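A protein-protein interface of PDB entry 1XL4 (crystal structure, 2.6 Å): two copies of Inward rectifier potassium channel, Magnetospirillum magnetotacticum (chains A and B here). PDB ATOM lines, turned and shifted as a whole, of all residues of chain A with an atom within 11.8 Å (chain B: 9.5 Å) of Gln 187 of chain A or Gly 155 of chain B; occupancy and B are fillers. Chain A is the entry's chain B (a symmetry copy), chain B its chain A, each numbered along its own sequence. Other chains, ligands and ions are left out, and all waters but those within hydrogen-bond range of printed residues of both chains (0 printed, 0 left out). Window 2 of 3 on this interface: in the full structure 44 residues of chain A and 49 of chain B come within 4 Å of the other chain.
The side-chain carboxylate (OE1) of Glu 154 of chain B sits at hydrogen-bond distance from the backbone NH (N) of Gln 187 of chain A, 3.0 Å away.
The side-chain carboxylate of Glu 188 of chain A sits at hydrogen-bond distance from the backbone NH of Glu 154 of chain B, at 2.7 Å.
The side-chain carboxylate (OE2) of Glu 154 of chain B lies within salt-bridge range of the guanidinium group (NH1) of Arg 194 of chain A, at 3.4 Å.
N of Gly 155 of chain B sits at hydrogen-bond distance from OE2 of Glu 188 of chain A (2.6 Å).
OE1 of Glu 154 of chain B touches CA of Ser 186 of chain A, at 3.1 Å.
OE1 of Gln 187 of chain A touches CA of Gly 155 of chain B, at 3.8 Å.
Glu 188 of chain A touches Asp 152 of chain B.
Glu 188 of chain A touches Phe 153 of chain B (OE1 to CA, 3.4 Å).
CZ of Phe 192 of chain A touches CZ of Phe 153 of chain B, at 3.7 Å.
CZ of Phe 153 of chain B touches NH1 of Arg 194 of chain A (3.8 Å).
No position is printed for both chains.
Ile 185 of chain A touches none of the printed residues of chain B.
Gln 187 of chain A touches just these residues of chain B: Glu 154 (3.0 Å) and Gly 155 (3.8 Å).
Of the printed residues of chain B, Phe 192 of chain A touches Phe 153 (3.7 Å).
Printed residues of chain B within 4 Å of Arg 194 of chain A: Phe 153 (3.8 Å) and Glu 154 (3.4 Å).
Phe 153 of chain B touches three residues of chain A.
Gly 155 of chain B touches just these residues of chain A: Gln 187 (3.8 Å) and Glu 188 (2.6 Å).
No residue of chain A comes within 4 Å of Pro 157 of chain B.
Thr 158 of chain B touches none of the printed residues of chain A.
The nearest residue of chain A that does not touch Gly 155 of chain B is Ser 186 of chain A (6.6 Å).
Hydrophobic or aromatic side chains of chain B that line the printed part of chain A: Phe 153.
Among the printed residues, 10 pairs touch across the chains.
Among the printed residues, Asp or Glu carboxylates within 4 Å of a Lys or Arg side-chain nitrogen of the other chain: Arg 194 of chain A with Glu 154 of chain B.
The backbone carbonyl oxygen of Phe 192 of chain A sits at hydrogen-bond distance from the backbone NH of Glu 184 of chain A, 2.9 Å away.
The side-chain hydroxyl of Ser 186 of chain A sits at hydrogen-bond distance from the side-chain carboxylate of Glu 188 of chain A, 3.2 Å away.
The backbone NH (N) of Gly 189 of chain A sits at hydrogen-bond distance from the side-chain hydroxyl (OG) of Ser 186 of chain A, at 3.5 Å.
N of Met 190 of chain A is in hydrogen-bond range of OG of Ser 186 of chain A (3.1 Å).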
ATOM      1  N   SER A 183     -10.892 -12.741   5.093  1.00  0.00           N
ATOM      2  CA  SER A 183      -9.673 -13.490   4.818  1.00  0.00           C
ATOM      3  C   SER A 183      -8.443 -12.624   4.994  1.00  0.00           C
ATOM      4  O   SER A 183      -8.356 -11.535   4.424  1.00  0.00           O
ATOM      5  CB  SER A 183      -9.718 -14.037   3.396  1.00  0.00           C
ATOM      6  OG  SER A 183     -10.869 -14.837   3.202  1.00  0.00           O
ATOM      7  N   GLU A 184      -7.498 -13.115   5.786  1.00  0.00           N
ATOM      8  CA  GLU A 184      -6.254 -12.401   6.047  1.00  0.00           C
ATOM      9  C   GLU A 184      -5.052 -13.325   5.849  1.00  0.00           C
ATOM     10  O   GLU A 184      -5.194 -14.550   5.830  1.00  0.00           O
ATOM     11  CB  GLU A 184      -6.278 -11.822   7.464  1.00  0.00           C
ATOM     12  CG  GLU A 184      -7.297 -10.693   7.605  1.00  0.00           C
ATOM     13  CD  GLU A 184      -7.484 -10.191   9.036  1.00  0.00           C
ATOM     14  OE1 GLU A 184      -6.480  -9.876   9.709  1.00  0.00           O
ATOM     15  OE2 GLU A 184      -8.650 -10.096   9.479  1.00  0.00           O
ATOM     16  N   ILE A 185      -3.870 -12.737   5.693  1.00  0.00           N
ATOM     17  CA  ILE A 185      -2.649 -13.513   5.471  1.00  0.00           C
ATOM     18  C   ILE A 185      -1.715 -13.502   6.686  1.00  0.00           C
ATOM     19  O   ILE A 185      -1.381 -12.432   7.209  1.00  0.00           O
ATOM     20  CB  ILE A 185      -1.870 -12.949   4.262  1.00  0.00           C
ATOM     21  CG1 ILE A 185      -2.843 -12.611   3.131  1.00  0.00           C
ATOM     22  CG2 ILE A 185      -0.821 -13.963   3.802  1.00  0.00           C
ATOM     23  CD1 ILE A 185      -2.234 -11.782   2.023  1.00  0.00           C
ATOM     24  N   SER A 186      -1.285 -14.682   7.129  1.00  0.00           N
ATOM     25  CA  SER A 186      -0.381 -14.767   8.276  1.00  0.00           C
ATOM     26  C   SER A 186       1.029 -14.424   7.824  1.00  0.00           C
ATOM     27  O   SER A 186       1.256 -14.155   6.645  1.00  0.00           O
ATOM     28  CB  SER A 186      -0.391 -16.175   8.885  1.00  0.00           C
ATOM     29  OG  SER A 186       0.321 -17.106   8.084  1.00  0.00           O
ATOM     30  N   GLN A 187       1.974 -14.419   8.757  1.00  0.00           N
ATOM     31  CA  GLN A 187       3.360 -14.132   8.410  1.00  0.00           C
ATOM     32  C   GLN A 187       3.925 -15.315   7.633  1.00  0.00           C
ATOM     33  O   GLN A 187       4.686 -15.143   6.685  1.00  0.00           O
ATOM     34  CB  GLN A 187       4.194 -13.887   9.667  1.00  0.00           C
ATOM     35  CG  GLN A 187       3.995 -12.510  10.269  1.00  0.00           C
ATOM     36  CD  GLN A 187       4.876 -12.278  11.479  1.00  0.00           C
ATOM     37  OE1 GLN A 187       6.057 -12.635  11.474  1.00  0.00           O
ATOM     38  NE2 GLN A 187       4.313 -11.670  12.520  1.00  0.00           N
ATOM     39  N   GLU A 188       3.533 -16.519   8.037  1.00  0.00           N
ATOM     40  CA  GLU A 188       3.986 -17.734   7.371  1.00  0.00           C
ATOM     41  C   GLU A 188       3.415 -17.778   5.958  1.00  0.00           C
ATOM     42  O   GLU A 188       3.580 -18.766   5.246  1.00  0.00           O
ATOM     43  CB  GLU A 188       3.527 -18.974   8.145  1.00  0.00           C
ATOM     44  CG  GLU A 188       4.059 -19.089   9.574  1.00  0.00           C
ATOM     45  CD  GLU A 188       3.594 -17.959  10.481  1.00  0.00           C
ATOM     46  OE1 GLU A 188       2.391 -17.611  10.440  1.00  0.00           O
ATOM     47  OE2 GLU A 188       4.433 -17.431  11.247  1.00  0.00           O
ATOM     48  N   GLY A 189       2.719 -16.712   5.571  1.00  0.00           N
ATOM     49  CA  GLY A 189       2.140 -16.636   4.239  1.00  0.00           C
ATOM     50  C   GLY A 189       0.795 -17.315   4.037  1.00  0.00           C
ATOM     51  O   GLY A 189       0.241 -17.271   2.939  1.00  0.00           O
ATOM     52  N   MET A 190       0.263 -17.940   5.084  1.00  0.00           N
ATOM     53  CA  MET A 190      -1.025 -18.621   4.988  1.00  0.00           C
ATOM     54  C   MET A 190      -2.233 -17.673   5.029  1.00  0.00           C
ATOM     55  O   MET A 190      -2.295 -16.752   5.851  1.00  0.00           O
ATOM     56  CB  MET A 190      -1.158 -19.651   6.113  1.00  0.00           C
ATOM     57  CG  MET A 190      -2.540 -20.279   6.211  1.00  0.00           C
ATOM     58  SD  MET A 190      -2.683 -21.474   7.556  1.00  0.00           S
ATOM     59  CE  MET A 190      -2.956 -20.380   8.970  1.00  0.00           C
ATOM     60  N   VAL A 191      -3.189 -17.904   4.131  1.00  0.00           N
ATOM     61  CA  VAL A 191      -4.402 -17.093   4.074  1.00  0.00           C
ATOM     62  C   VAL A 191      -5.529 -17.881   4.730  1.00  0.00           C
ATOM     63  O   VAL A 191      -5.895 -18.962   4.266  1.00  0.00           O
ATOM     64  CB  VAL A 191      -4.795 -16.756   2.621  1.00  0.00           C
ATOM     65  CG1 VAL A 191      -6.163 -16.083   2.597  1.00  0.00           C
ATOM     66  CG2 VAL A 191      -3.754 -15.837   2.008  1.00  0.00           C
ATOM     67  N   PHE A 192      -6.071 -17.326   5.812  1.00  0.00           N
ATOM     68  CA  PHE A 192      -7.139 -17.968   6.573  1.00  0.00           C
ATOM     69  C   PHE A 192      -8.240 -16.967   6.927  1.00  0.00           C
ATOM     70  O   PHE A 192      -8.063 -15.756   6.785  1.00  0.00           O
ATOM     71  CB  PHE A 192      -6.546 -18.549   7.855  1.00  0.00           C
ATOM     72  CG  PHE A 192      -5.959 -17.509   8.768  1.00  0.00           C
ATOM     73  CD1 PHE A 192      -6.712 -16.979   9.820  1.00  0.00           C
ATOM     74  CD2 PHE A 192      -4.678 -17.016   8.547  1.00  0.00           C
ATOM     75  CE1 PHE A 192      -6.195 -15.968  10.638  1.00  0.00           C
ATOM     76  CE2 PHE A 192      -4.153 -16.005   9.358  1.00  0.00           C
ATOM     77  CZ  PHE A 192      -4.914 -15.480  10.405  1.00  0.00           C
ATOM     78  N   ARG A 194     -10.213 -14.876   9.426  1.00  0.00           N
ATOM     79  CA  ARG A 194     -10.049 -14.323  10.760  1.00  0.00           C
ATOM     80  C   ARG A 194     -11.376 -13.747  11.253  1.00  0.00           C
ATOM     81  O   ARG A 194     -12.169 -13.204  10.478  1.00  0.00           O
ATOM     82  CB  ARG A 194      -8.970 -13.236  10.754  1.00  0.00           C
ATOM     83  CG  ARG A 194      -8.583 -12.734  12.142  1.00  0.00           C
ATOM     84  CD  ARG A 194      -7.094 -12.946  12.441  1.00  0.00           C
ATOM     85  NE  ARG A 194      -6.889 -13.832  13.590  1.00  0.00           N
ATOM     86  CZ  ARG A 194      -5.697 -14.190  14.067  1.00  0.00           C
ATOM     87  NH1 ARG A 194      -4.588 -13.739  13.493  1.00  0.00           N
ATOM     88  NH2 ARG A 194      -5.615 -14.991  15.124  1.00  0.00           N
ATOM     89  N   SER B 151       4.156 -25.079  16.612  1.00  0.00           N
ATOM     90  CA  SER B 151       4.856 -24.575  15.445  1.00  0.00           C
ATOM     91  C   SER B 151       4.498 -23.104  15.235  1.00  0.00           C
ATOM     92  O   SER B 151       3.619 -22.572  15.908  1.00  0.00           O
ATOM     93  CB  SER B 151       4.507 -25.411  14.215  1.00  0.00           C
ATOM     94  OG  SER B 151       3.120 -25.396  13.957  1.00  0.00           O
ATOM     95  N   ASP B 152       5.176 -22.454  14.296  1.00  0.00           N
ATOM     96  CA  ASP B 152       4.974 -21.037  14.021  1.00  0.00           C
ATOM     97  C   ASP B 152       3.661 -20.560  13.410  1.00  0.00           C
ATOM     98  O   ASP B 152       3.192 -21.087  12.402  1.00  0.00           O
ATOM     99  CB  ASP B 152       6.107 -20.521  13.135  1.00  0.00           C
ATOM    100  CG  ASP B 152       7.423 -20.406  13.870  1.00  0.00           C
ATOM    101  OD1 ASP B 152       8.432 -20.065  13.217  1.00  0.00           O
ATOM    102  OD2 ASP B 152       7.455 -20.648  15.091  1.00  0.00           O
ATOM    103  N   PHE B 153       3.088 -19.542  14.045  1.00  0.00           N
ATOM    104  CA  PHE B 153       1.880 -18.873  13.578  1.00  0.00           C
ATOM    105  C   PHE B 153       2.121 -17.402  13.903  1.00  0.00           C
ATOM    106  O   PHE B 153       2.358 -17.047  15.058  1.00  0.00           O
ATOM    107  CB  PHE B 153       0.622 -19.347  14.299  1.00  0.00           C
ATOM    108  CG  PHE B 153      -0.624 -18.602  13.875  1.00  0.00           C
ATOM    109  CD1 PHE B 153      -1.090 -18.690  12.563  1.00  0.00           C
ATOM    110  CD2 PHE B 153      -1.308 -17.781  14.776  1.00  0.00           C
ATOM    111  CE1 PHE B 153      -2.220 -17.967  12.148  1.00  0.00           C
ATOM    112  CE2 PHE B 153      -2.436 -17.054  14.373  1.00  0.00           C
ATOM    113  CZ  PHE B 153      -2.894 -17.148  13.055  1.00  0.00           C
ATOM    114  N   GLU B 154       2.073 -16.551  12.881  1.00  0.00           N
ATOM    115  CA  GLU B 154       2.320 -15.130  13.068  1.00  0.00           C
ATOM    116  C   GLU B 154       3.717 -14.933  13.655  1.00  0.00           C
ATOM    117  O   GLU B 154       3.934 -14.053  14.490  1.00  0.00           O
ATOM    118  CB  GLU B 154       1.275 -14.521  14.004  1.00  0.00           C
ATOM    119  CG  GLU B 154      -0.152 -14.692  13.524  1.00  0.00           C
ATOM    120  CD  GLU B 154      -0.437 -13.954  12.234  1.00  0.00           C
ATOM    121  OE1 GLU B 154       0.330 -14.117  11.264  1.00  0.00           O
ATOM    122  OE2 GLU B 154      -1.440 -13.214  12.191  1.00  0.00           O
ATOM    123  N   GLY B 155       4.655 -15.775  13.225  1.00  0.00           N
ATOM    124  CA  GLY B 155       6.029 -15.674  13.684  1.00  0.00           C
ATOM    125  C   GLY B 155       6.340 -16.133  15.095  1.00  0.00           C
ATOM    126  O   GLY B 155       7.423 -15.851  15.603  1.00  0.00           O
ATOM    127  N   LYS B 156       5.418 -16.841  15.738  1.00  0.00           N
ATOM    128  CA  LYS B 156       5.653 -17.318  17.098  1.00  0.00           C
ATOM    129  C   LYS B 156       5.329 -18.792  17.305  1.00  0.00           C
ATOM    130  O   LYS B 156       4.387 -19.323  16.712  1.00  0.00           O
ATOM    131  CB  LYS B 156       4.819 -16.521  18.100  1.00  0.00           C
ATOM    132  CG  LYS B 156       5.223 -15.091  18.284  1.00  0.00           C
ATOM    133  CD  LYS B 156       4.280 -14.411  19.260  1.00  0.00           C
ATOM    134  CE  LYS B 156       4.565 -12.921  19.355  1.00  0.00           C
ATOM    135  NZ  LYS B 156       3.440 -12.192  20.004  1.00  0.00           N
ATOM    136  N   PRO B 157       6.115 -19.477  18.152  1.00  0.00           N
ATOM    137  CA  PRO B 157       5.834 -20.890  18.403  1.00  0.00           C
ATOM    138  C   PRO B 157       4.431 -20.898  19.017  1.00  0.00           C
ATOM    139  O   PRO B 157       4.150 -20.127  19.934  1.00  0.00           O
ATOM    140  CB  PRO B 157       6.911 -21.278  19.410  1.00  0.00           C
ATOM    141  CG  PRO B 157       8.053 -20.355  19.061  1.00  0.00           C
ATOM    142  CD  PRO B 157       7.351 -19.049  18.831  1.00  0.00           C
ATOM    143  N   THR B 158       3.555 -21.760  18.517  1.00  0.00           N
ATOM    144  CA  THR B 158       2.185 -21.809  19.001  1.00  0.00           C
ATOM    145  C   THR B 158       1.716 -23.233  19.282  1.00  0.00           C
ATOM    146  O   THR B 158       1.855 -24.135  18.443  1.00  0.00           O
ATOM    147  CB  THR B 158       1.226 -21.172  17.957  1.00  0.00           C
ATOM    148  OG1 THR B 158       1.690 -19.861  17.623  1.00  0.00           O
ATOM    149  CG2 THR B 158      -0.190 -21.071  18.499  1.00  0.00           C
ATOM    150  N   MET B 160      -0.963 -25.873  19.431  1.00  0.00           N
ATOM    151  CA  MET B 160      -2.208 -25.996  18.695  1.00  0.00           C
ATOM    152  C   MET B 160      -2.839 -27.363  18.851  1.00  0.00           C
ATOM    153  O   MET B 160      -2.179 -28.321  19.218  1.00  0.00           O
ATOM    154  CB  MET B 160      -1.962 -25.747  17.204  1.00  0.00           C
ATOM    155  CG  MET B 160      -1.339 -24.403  16.837  1.00  0.00           C
ATOM    156  SD  MET B 160      -1.329 -24.189  15.015  1.00  0.00           S
ATOM    157  CE  MET B 160       0.251 -23.474  14.761  1.00  0.00           C
ATOM    158  N   PRO B 217      -0.451 -18.793  21.469  1.00  0.00           N
ATOM    159  CA  PRO B 217       0.904 -18.318  21.187  1.00  0.00           C
ATOM    160  C   PRO B 217       1.758 -18.435  22.440  1.00  0.00           C
ATOM    161  O   PRO B 217       1.324 -18.079  23.535  1.00  0.00           O
ATOM    162  CB  PRO B 217       0.680 -16.866  20.774  1.00  0.00           C
ATOM    163  CG  PRO B 217      -0.685 -16.891  20.180  1.00  0.00           C
ATOM    164  CD  PRO B 217      -1.441 -17.749  21.159  1.00  0.00           C
ATOM    165  N   ILE B 218       2.972 -18.940  22.283  1.00  0.00           N
ATOM    166  CA  ILE B 218       3.855 -19.080  23.416  1.00  0.00           C
ATOM    167  C   ILE B 218       4.735 -17.847  23.528  1.00  0.00           C
ATOM    168  O   ILE B 218       5.906 -17.881  23.174  1.00  0.00           O
ATOM    169  CB  ILE B 218       4.724 -20.339  23.278  1.00  0.00           C
ATOM    170  CG1 ILE B 218       3.810 -21.554  23.069  1.00  0.00           C
ATOM    171  CG2 ILE B 218       5.574 -20.535  24.537  1.00  0.00           C
ATOM    172  CD1 ILE B 218       4.526 -22.841  22.736  1.00  0.00           C
ATOM    173  N   ASP B 219       4.155 -16.753  24.017  1.00  0.00           N
ATOM    174  CA  ASP B 219       4.886 -15.502  24.195  1.00  0.00           C
ATOM    175  C   ASP B 219       5.381 -15.410  25.642  1.00  0.00           C
ATOM    176  O   ASP B 219       5.128 -16.314  26.439  1.00  0.00           O
ATOM    177  CB  ASP B 219       3.986 -14.307  23.838  1.00  0.00           C
ATOM    178  CG  ASP B 219       2.802 -14.152  24.785  1.00  0.00           C
ATOM    179  OD1 ASP B 219       1.859 -13.408  24.436  1.00  0.00           O
ATOM    180  OD2 ASP B 219       2.812 -14.761  25.879  1.00  0.00           O
